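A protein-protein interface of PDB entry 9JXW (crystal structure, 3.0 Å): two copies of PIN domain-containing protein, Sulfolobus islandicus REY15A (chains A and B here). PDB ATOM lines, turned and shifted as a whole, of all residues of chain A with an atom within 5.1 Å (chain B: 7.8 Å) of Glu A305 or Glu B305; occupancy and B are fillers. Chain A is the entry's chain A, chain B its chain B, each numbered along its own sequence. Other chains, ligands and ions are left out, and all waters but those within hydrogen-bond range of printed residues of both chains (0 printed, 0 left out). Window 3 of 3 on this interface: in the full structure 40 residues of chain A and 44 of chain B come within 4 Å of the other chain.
The side-chain amide oxygen (OD1) of Asn A309 sits close to the side-chain carboxylate (OD1) of Asp B296 (3.3 Å). OE1 of Glu A302 sits close to O of Asn B309, 2.8 Å away. The side-chain carboxylate (OE1) of Glu B305 lies close to the side-chain carboxylate (OE1) of Glu A305, at 3.1 Å. The backbone carbonyl oxygen (O) of Asn A309 lies close to the side-chain carboxylate (OE1) of Glu B302, 2.8 Å away.
NZ of Lys A308 lies within salt-bridge range of OE1 of Glu A305 (3.9 Å). The backbone carbonyl oxygen (O) of Glu A305 lies within hydrogen-bond range of the side-chain amide nitrogen (ND2) of Asn A309. N of Gly B298 sits close to OD1 of Asp B296 (3.5 Å). The side-chain carboxylate (OD2) of Asp B296 sits close to the side-chain carboxylate (OE1) of Glu B302 (2.7 Å). ND2 of Asn B309 is in hydrogen-bond range of O of Glu B305, at 2.5 Å.
Among the printed residues, merely in contact across the chains: Glu A305 with Asn B309, Ile A306 with Val B310 and Asn A309 with Glu B305.
Of the printed residues of chain A, Asp B296 touches Asn A309. Of the printed residues of chain B, Ile A306 touches Val B310. Of the printed residues of chain A, Val B310 touches Ile A306. Printed residues of chain B within 4 Å of Asn A309: Asp B296 (3.3 Å), Glu B302 (2.8 Å) and Glu B305 (3.6 Å). Val B314 touches none of the printed residues of chain A. The nearest printed residue of chain A that does not touch Glu B302 is Lys A308 (6.0 Å).
Of the 9 printed residues of chain A, 4 touch a printed residue of chain B. Hydrophobic or aromatic side chains of chain A that line the printed part of chain B: Ile A306. Among the printed residues, 7 pairs touch across the chains. Among the printed residues, no Asp or Glu carboxylate lies within 4 Å of a Lys or Arg side-chain nitrogen of the other chain.
Glu A302 touches Asn B309, and with the chains exchanged Asn A309 touches Glu B302. Glu A305 touches its own counterpart, Glu B305. Glu A305 touches Asn B309, and with the chains exchanged Asn A309 touches Glu B305. 9 positions are printed for both chains. Of the 7 pairs that touch across the chains among the printed residues, 5 have their exchanged pair printed and touching as well.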
ATOM      1  N   ASN A 301       7.979  17.507  35.450  1.00  0.00           N
ATOM      2  CA  ASN A 301       8.311  17.526  34.027  1.00  0.00           C
ATOM      3  C   ASN A 301       9.534  18.392  33.756  1.00  0.00           C
ATOM      4  O   ASN A 301      10.414  18.002  32.979  1.00  0.00           O
ATOM      5  CB  ASN A 301       7.116  18.011  33.203  1.00  0.00           C
ATOM      6  CG  ASN A 301       7.283  17.747  31.705  1.00  0.00           C
ATOM      7  OD1 ASN A 301       6.340  17.905  30.933  1.00  0.00           O
ATOM      8  ND2 ASN A 301       8.471  17.317  31.299  1.00  0.00           N
ATOM      9  N   GLU A 302       9.616  19.566  34.387  1.00  0.00           N
ATOM     10  CA  GLU A 302      10.756  20.438  34.134  1.00  0.00           C
ATOM     11  C   GLU A 302      12.052  19.816  34.642  1.00  0.00           C
ATOM     12  O   GLU A 302      13.109  20.012  34.033  1.00  0.00           O
ATOM     13  CB  GLU A 302      10.521  21.820  34.752  1.00  0.00           C
ATOM     14  CG  GLU A 302      10.316  21.837  36.254  1.00  0.00           C
ATOM     15  CD  GLU A 302       9.806  23.175  36.760  1.00  0.00           C
ATOM     16  OE1 GLU A 302       9.594  24.087  35.934  1.00  0.00           O
ATOM     17  OE2 GLU A 302       9.619  23.321  37.983  1.00  0.00           O
ATOM     18  N   ALA A 303      11.990  19.053  35.736  1.00  0.00           N
ATOM     19  CA  ALA A 303      13.167  18.317  36.186  1.00  0.00           C
ATOM     20  C   ALA A 303      13.581  17.262  35.168  1.00  0.00           C
ATOM     21  O   ALA A 303      14.775  17.081  34.902  1.00  0.00           O
ATOM     22  CB  ALA A 303      12.897  17.677  37.548  1.00  0.00           C
ATOM     23  N   LEU A 304      12.608  16.557  34.582  1.00  0.00           N
ATOM     24  CA  LEU A 304      12.926  15.587  33.538  1.00  0.00           C
ATOM     25  C   LEU A 304      13.539  16.264  32.320  1.00  0.00           C
ATOM     26  O   LEU A 304      14.486  15.743  31.721  1.00  0.00           O
ATOM     27  CB  LEU A 304      11.671  14.815  33.123  1.00  0.00           C
ATOM     28  CG  LEU A 304      11.244  13.544  33.859  1.00  0.00           C
ATOM     29  CD1 LEU A 304      12.191  12.419  33.503  1.00  0.00           C
ATOM     30  CD2 LEU A 304      11.203  13.734  35.355  1.00  0.00           C
ATOM     31  N   GLU A 305      12.993  17.414  31.923  1.00  0.00           N
ATOM     32  CA  GLU A 305      13.497  18.106  30.742  1.00  0.00           C
ATOM     33  C   GLU A 305      14.931  18.587  30.943  1.00  0.00           C
ATOM     34  O   GLU A 305      15.750  18.524  30.019  1.00  0.00           O
ATOM     35  CB  GLU A 305      12.565  19.261  30.382  1.00  0.00           C
ATOM     36  CG  GLU A 305      11.160  18.815  29.971  1.00  0.00           C
ATOM     37  CD  GLU A 305      11.074  18.395  28.515  1.00  0.00           C
ATOM     38  OE1 GLU A 305      12.136  18.268  27.872  1.00  0.00           O
ATOM     39  OE2 GLU A 305       9.944  18.210  28.011  1.00  0.00           O
ATOM     40  N   ILE A 306      15.243  19.118  32.129  1.00  0.00           N
ATOM     41  CA  ILE A 306      16.614  19.533  32.409  1.00  0.00           C
ATOM     42  C   ILE A 306      17.523  18.315  32.511  1.00  0.00           C
ATOM     43  O   ILE A 306      18.673  18.340  32.055  1.00  0.00           O
ATOM     44  CB  ILE A 306      16.663  20.382  33.690  1.00  0.00           C
ATOM     45  CG1 ILE A 306      15.789  21.627  33.532  1.00  0.00           C
ATOM     46  CG2 ILE A 306      18.099  20.765  34.029  1.00  0.00           C
ATOM     47  CD1 ILE A 306      15.698  22.469  34.784  1.00  0.00           C
ATOM     48  N   LYS A 307      17.017  17.230  33.104  1.00  0.00           N
ATOM     49  CA  LYS A 307      17.813  16.019  33.270  1.00  0.00           C
ATOM     50  C   LYS A 307      18.205  15.420  31.924  1.00  0.00           C
ATOM     51  O   LYS A 307      19.343  14.968  31.745  1.00  0.00           O
ATOM     52  CB  LYS A 307      17.044  14.997  34.107  1.00  0.00           C
ATOM     53  CG  LYS A 307      17.895  13.852  34.631  1.00  0.00           C
ATOM     54  CD  LYS A 307      17.037  12.688  35.107  1.00  0.00           C
ATOM     55  CE  LYS A 307      17.837  11.726  35.974  1.00  0.00           C
ATOM     56  NZ  LYS A 307      18.155  12.309  37.308  1.00  0.00           N
ATOM     57  N   LYS A 308      17.279  15.410  30.964  1.00  0.00           N
ATOM     58  CA  LYS A 308      17.523  14.784  29.671  1.00  0.00           C
ATOM     59  C   LYS A 308      18.405  15.619  28.757  1.00  0.00           C
ATOM     60  O   LYS A 308      18.840  15.117  27.714  1.00  0.00           O
ATOM     61  CB  LYS A 308      16.195  14.523  28.954  1.00  0.00           C
ATOM     62  CG  LYS A 308      15.520  15.802  28.480  1.00  0.00           C
ATOM     63  CD  LYS A 308      14.460  15.561  27.415  1.00  0.00           C
ATOM     64  CE  LYS A 308      13.317  14.704  27.932  1.00  0.00           C
ATOM     65  NZ  LYS A 308      12.286  14.484  26.880  1.00  0.00           N
ATOM     66  N   ASN A 309      18.682  16.871  29.116  1.00  0.00           N
ATOM     67  CA  ASN A 309      19.454  17.760  28.264  1.00  0.00           C
ATOM     68  C   ASN A 309      20.811  18.129  28.838  1.00  0.00           C
ATOM     69  O   ASN A 309      21.657  18.639  28.097  1.00  0.00           O
ATOM     70  CB  ASN A 309      18.658  19.041  27.985  1.00  0.00           C
ATOM     71  CG  ASN A 309      17.533  18.820  26.998  1.00  0.00           C
ATOM     72  OD1 ASN A 309      17.771  18.543  25.821  1.00  0.00           O
ATOM     73  ND2 ASN A 309      16.298  18.929  27.472  1.00  0.00           N
ATOM     74  N   LEU B 218      25.089  27.637  28.182  1.00  0.00           N
ATOM     75  CA  LEU B 218      25.297  26.368  27.495  1.00  0.00           C
ATOM     76  C   LEU B 218      26.340  26.595  26.414  1.00  0.00           C
ATOM     77  O   LEU B 218      26.161  27.457  25.547  1.00  0.00           O
ATOM     78  CB  LEU B 218      23.993  25.838  26.894  1.00  0.00           C
ATOM     79  CG  LEU B 218      23.000  25.204  27.869  1.00  0.00           C
ATOM     80  CD1 LEU B 218      21.731  24.794  27.145  1.00  0.00           C
ATOM     81  CD2 LEU B 218      23.626  24.001  28.557  1.00  0.00           C
ATOM     82  N   ASP B 296      20.682  13.207  22.146  1.00  0.00           N
ATOM     83  CA  ASP B 296      20.126  14.518  22.450  1.00  0.00           C
ATOM     84  C   ASP B 296      19.750  15.208  21.145  1.00  0.00           C
ATOM     85  O   ASP B 296      20.280  14.892  20.076  1.00  0.00           O
ATOM     86  CB  ASP B 296      21.120  15.354  23.267  1.00  0.00           C
ATOM     87  CG  ASP B 296      20.557  16.697  23.691  1.00  0.00           C
ATOM     88  OD1 ASP B 296      19.372  16.976  23.412  1.00  0.00           O
ATOM     89  OD2 ASP B 296      21.306  17.474  24.315  1.00  0.00           O
ATOM     90  N   MET B 297      18.824  16.169  21.247  1.00  0.00           N
ATOM     91  CA  MET B 297      18.303  16.869  20.079  1.00  0.00           C
ATOM     92  C   MET B 297      19.155  18.049  19.627  1.00  0.00           C
ATOM     93  O   MET B 297      18.835  18.657  18.600  1.00  0.00           O
ATOM     94  CB  MET B 297      16.884  17.366  20.366  1.00  0.00           C
ATOM     95  CG  MET B 297      15.890  17.045  19.272  1.00  0.00           C
ATOM     96  SD  MET B 297      15.713  15.265  19.084  1.00  0.00           S
ATOM     97  CE  MET B 297      15.238  14.802  20.751  1.00  0.00           C
ATOM     98  N   GLY B 298      20.208  18.403  20.350  1.00  0.00           N
ATOM     99  CA  GLY B 298      21.116  19.446  19.918  1.00  0.00           C
ATOM    100  C   GLY B 298      21.245  20.559  20.943  1.00  0.00           C
ATOM    101  O   GLY B 298      20.462  20.683  21.882  1.00  0.00           O
ATOM    102  N   LEU B 299      22.269  21.388  20.720  1.00  0.00           N
ATOM    103  CA  LEU B 299      22.549  22.497  21.627  1.00  0.00           C
ATOM    104  C   LEU B 299      21.426  23.529  21.623  1.00  0.00           C
ATOM    105  O   LEU B 299      21.082  24.086  22.673  1.00  0.00           O
ATOM    106  CB  LEU B 299      23.876  23.152  21.251  1.00  0.00           C
ATOM    107  CG  LEU B 299      24.371  24.262  22.176  1.00  0.00           C
ATOM    108  CD1 LEU B 299      24.835  23.695  23.508  1.00  0.00           C
ATOM    109  CD2 LEU B 299      25.480  25.052  21.507  1.00  0.00           C
ATOM    110  N   ILE B 300      20.868  23.827  20.448  1.00  0.00           N
ATOM    111  CA  ILE B 300      19.779  24.798  20.375  1.00  0.00           C
ATOM    112  C   ILE B 300      18.537  24.265  21.077  1.00  0.00           C
ATOM    113  O   ILE B 300      17.881  24.985  21.840  1.00  0.00           O
ATOM    114  CB  ILE B 300      19.484  25.172  18.911  1.00  0.00           C
ATOM    115  CG1 ILE B 300      20.681  25.897  18.296  1.00  0.00           C
ATOM    116  CG2 ILE B 300      18.230  26.028  18.820  1.00  0.00           C
ATOM    117  CD1 ILE B 300      20.441  26.367  16.881  1.00  0.00           C
ATOM    118  N   ASN B 301      18.194  22.998  20.832  1.00  0.00           N
ATOM    119  CA  ASN B 301      16.974  22.439  21.405  1.00  0.00           C
ATOM    120  C   ASN B 301      17.037  22.399  22.926  1.00  0.00           C
ATOM    121  O   ASN B 301      16.058  22.733  23.601  1.00  0.00           O
ATOM    122  CB  ASN B 301      16.725  21.039  20.844  1.00  0.00           C
ATOM    123  CG  ASN B 301      15.340  20.521  21.171  1.00  0.00           C
ATOM    124  OD1 ASN B 301      15.143  19.827  22.169  1.00  0.00           O
ATOM    125  ND2 ASN B 301      14.368  20.864  20.332  1.00  0.00           N
ATOM    126  N   GLU B 302      18.181  21.993  23.485  1.00  0.00           N
ATOM    127  CA  GLU B 302      18.290  21.908  24.937  1.00  0.00           C
ATOM    128  C   GLU B 302      18.230  23.282  25.590  1.00  0.00           C
ATOM    129  O   GLU B 302      17.677  23.419  26.687  1.00  0.00           O
ATOM    130  CB  GLU B 302      19.572  21.175  25.333  1.00  0.00           C
ATOM    131  CG  GLU B 302      20.856  21.812  24.844  1.00  0.00           C
ATOM    132  CD  GLU B 302      22.056  20.906  25.034  1.00  0.00           C
ATOM    133  OE1 GLU B 302      21.878  19.784  25.547  1.00  0.00           O
ATOM    134  OE2 GLU B 302      23.177  21.309  24.668  1.00  0.00           O
ATOM    135  N   ALA B 303      18.779  24.310  24.937  1.00  0.00           N
ATOM    136  CA  ALA B 303      18.616  25.665  25.450  1.00  0.00           C
ATOM    137  C   ALA B 303      17.152  26.084  25.414  1.00  0.00           C
ATOM    138  O   ALA B 303      16.657  26.725  26.347  1.00  0.00           O
ATOM    139  CB  ALA B 303      19.479  26.643  24.653  1.00  0.00           C
ATOM    140  N   LEU B 304      16.445  25.732  24.338  1.00  0.00           N
ATOM    141  CA  LEU B 304      15.022  26.040  24.246  1.00  0.00           C
ATOM    142  C   LEU B 304      14.221  25.297  25.314  1.00  0.00           C
ATOM    143  O   LEU B 304      13.315  25.872  25.928  1.00  0.00           O
ATOM    144  CB  LEU B 304      14.506  25.713  22.842  1.00  0.00           C
ATOM    145  CG  LEU B 304      14.710  26.803  21.776  1.00  0.00           C
ATOM    146  CD1 LEU B 304      14.145  26.367  20.429  1.00  0.00           C
ATOM    147  CD2 LEU B 304      14.115  28.147  22.199  1.00  0.00           C
ATOM    148  N   GLU B 305      14.543  24.020  25.555  1.00  0.00           N
ATOM    149  CA  GLU B 305      13.808  23.252  26.559  1.00  0.00           C
ATOM    150  C   GLU B 305      13.991  23.843  27.948  1.00  0.00           C
ATOM    151  O   GLU B 305      13.020  23.994  28.697  1.00  0.00           O
ATOM    152  CB  GLU B 305      14.265  21.792  26.560  1.00  0.00           C
ATOM    153  CG  GLU B 305      13.967  21.026  25.288  1.00  0.00           C
ATOM    154  CD  GLU B 305      12.563  20.451  25.255  1.00  0.00           C
ATOM    155  OE1 GLU B 305      11.759  20.772  26.156  1.00  0.00           O
ATOM    156  OE2 GLU B 305      12.259  19.688  24.313  1.00  0.00           O
ATOM    157  N   ILE B 306      15.224  24.206  28.300  1.00  0.00           N
ATOM    158  CA  ILE B 306      15.485  24.794  29.609  1.00  0.00           C
ATOM    159  C   ILE B 306      14.871  26.187  29.711  1.00  0.00           C
ATOM    160  O   ILE B 306      14.377  26.580  30.774  1.00  0.00           O
ATOM    161  CB  ILE B 306      16.999  24.804  29.889  1.00  0.00           C
ATOM    162  CG1 ILE B 306      17.550  23.374  29.877  1.00  0.00           C
ATOM    163  CG2 ILE B 306      17.293  25.455  31.227  1.00  0.00           C
ATOM    164  CD1 ILE B 306      19.047  23.295  30.062  1.00  0.00           C
ATOM    165  N   LYS B 307      14.883  26.950  28.614  1.00  0.00           N
ATOM    166  CA  LYS B 307      14.362  28.314  28.655  1.00  0.00           C
ATOM    167  C   LYS B 307      12.884  28.337  29.030  1.00  0.00           C
ATOM    168  O   LYS B 307      12.455  29.164  29.844  1.00  0.00           O
ATOM    169  CB  LYS B 307      14.585  28.988  27.300  1.00  0.00           C
ATOM    170  CG  LYS B 307      14.416  30.497  27.289  1.00  0.00           C
ATOM    171  CD  LYS B 307      14.265  30.999  25.862  1.00  0.00           C
ATOM    172  CE  LYS B 307      14.489  32.497  25.772  1.00  0.00           C
ATOM    173  NZ  LYS B 307      15.922  32.857  25.966  1.00  0.00           N
ATOM    174  N   LYS B 308      12.091  27.431  28.462  1.00  0.00           N
ATOM    175  CA  LYS B 308      10.659  27.409  28.730  1.00  0.00           C
ATOM    176  C   LYS B 308      10.308  26.761  30.065  1.00  0.00           C
ATOM    177  O   LYS B 308       9.135  26.792  30.455  1.00  0.00           O
ATOM    178  CB  LYS B 308       9.913  26.698  27.599  1.00  0.00           C
ATOM    179  CG  LYS B 308      10.151  25.207  27.514  1.00  0.00           C
ATOM    180  CD  LYS B 308       9.048  24.546  26.707  1.00  0.00           C
ATOM    181  CE  LYS B 308       9.014  25.081  25.285  1.00  0.00           C
ATOM    182  NZ  LYS B 308       7.933  24.453  24.477  1.00  0.00           N
ATOM    183  N   ASN B 309      11.282  26.174  30.767  1.00  0.00           N
ATOM    184  CA  ASN B 309      11.022  25.464  32.011  1.00  0.00           C
ATOM    185  C   ASN B 309      11.578  26.151  33.253  1.00  0.00           C
ATOM    186  O   ASN B 309      11.184  25.782  34.364  1.00  0.00           O
ATOM    187  CB  ASN B 309      11.592  24.039  31.938  1.00  0.00           C
ATOM    188  CG  ASN B 309      10.769  23.123  31.049  1.00  0.00           C
ATOM    189  OD1 ASN B 309       9.622  22.807  31.358  1.00  0.00           O
ATOM    190  ND2 ASN B 309      11.356  22.688  29.940  1.00  0.00           N
ATOM    191  N   VAL B 310      12.474  27.129  33.108  1.00  0.00           N
ATOM    192  CA  VAL B 310      13.054  27.824  34.252  1.00  0.00           C
ATOM    193  C   VAL B 310      12.881  29.327  34.071  1.00  0.00           C
ATOM    194  O   VAL B 310      12.636  29.821  32.969  1.00  0.00           O
ATOM    195  CB  VAL B 310      14.549  27.480  34.456  1.00  0.00           C
ATOM    196  CG1 VAL B 310      14.761  25.973  34.450  1.00  0.00           C
ATOM    197  CG2 VAL B 310      15.410  28.153  33.393  1.00  0.00           C
ATOM    198  N   VAL B 314      18.658  31.916  29.948  1.00  0.00           N
ATOM    199  CA  VAL B 314      19.472  30.922  29.258  1.00  0.00           C
ATOM    200  C   VAL B 314      20.264  31.604  28.152  1.00  0.00           C
ATOM    201  O   VAL B 314      19.696  32.306  27.306  1.00  0.00           O
ATOM    202  CB  VAL B 314      18.597  29.789  28.697  1.00  0.00           C
ATOM    203  CG1 VAL B 314      19.451  28.795  27.935  1.00  0.00           C
ATOM    204  CG2 VAL B 314      17.853  29.098  29.827  1.00  0.00           C
ATOM    205  N   LEU B 332      16.695  32.688  21.225  1.00  0.00           N
ATOM    206  CA  LEU B 332      17.717  32.485  22.241  1.00  0.00           C
ATOM    207  C   LEU B 332      18.745  33.608  22.203  1.00  0.00           C
ATOM    208  O   LEU B 332      19.123  34.093  21.132  1.00  0.00           O
ATOM    209  CB  LEU B 332      18.415  31.140  22.034  1.00  0.00           C
ATOM    210  CG  LEU B 332      17.568  29.880  22.214  1.00  0.00           C
ATOM    211  CD1 LEU B 332      18.350  28.645  21.796  1.00  0.00           C
ATOM    212  CD2 LEU B 332      17.097  29.751  23.655  1.00  0.00           C
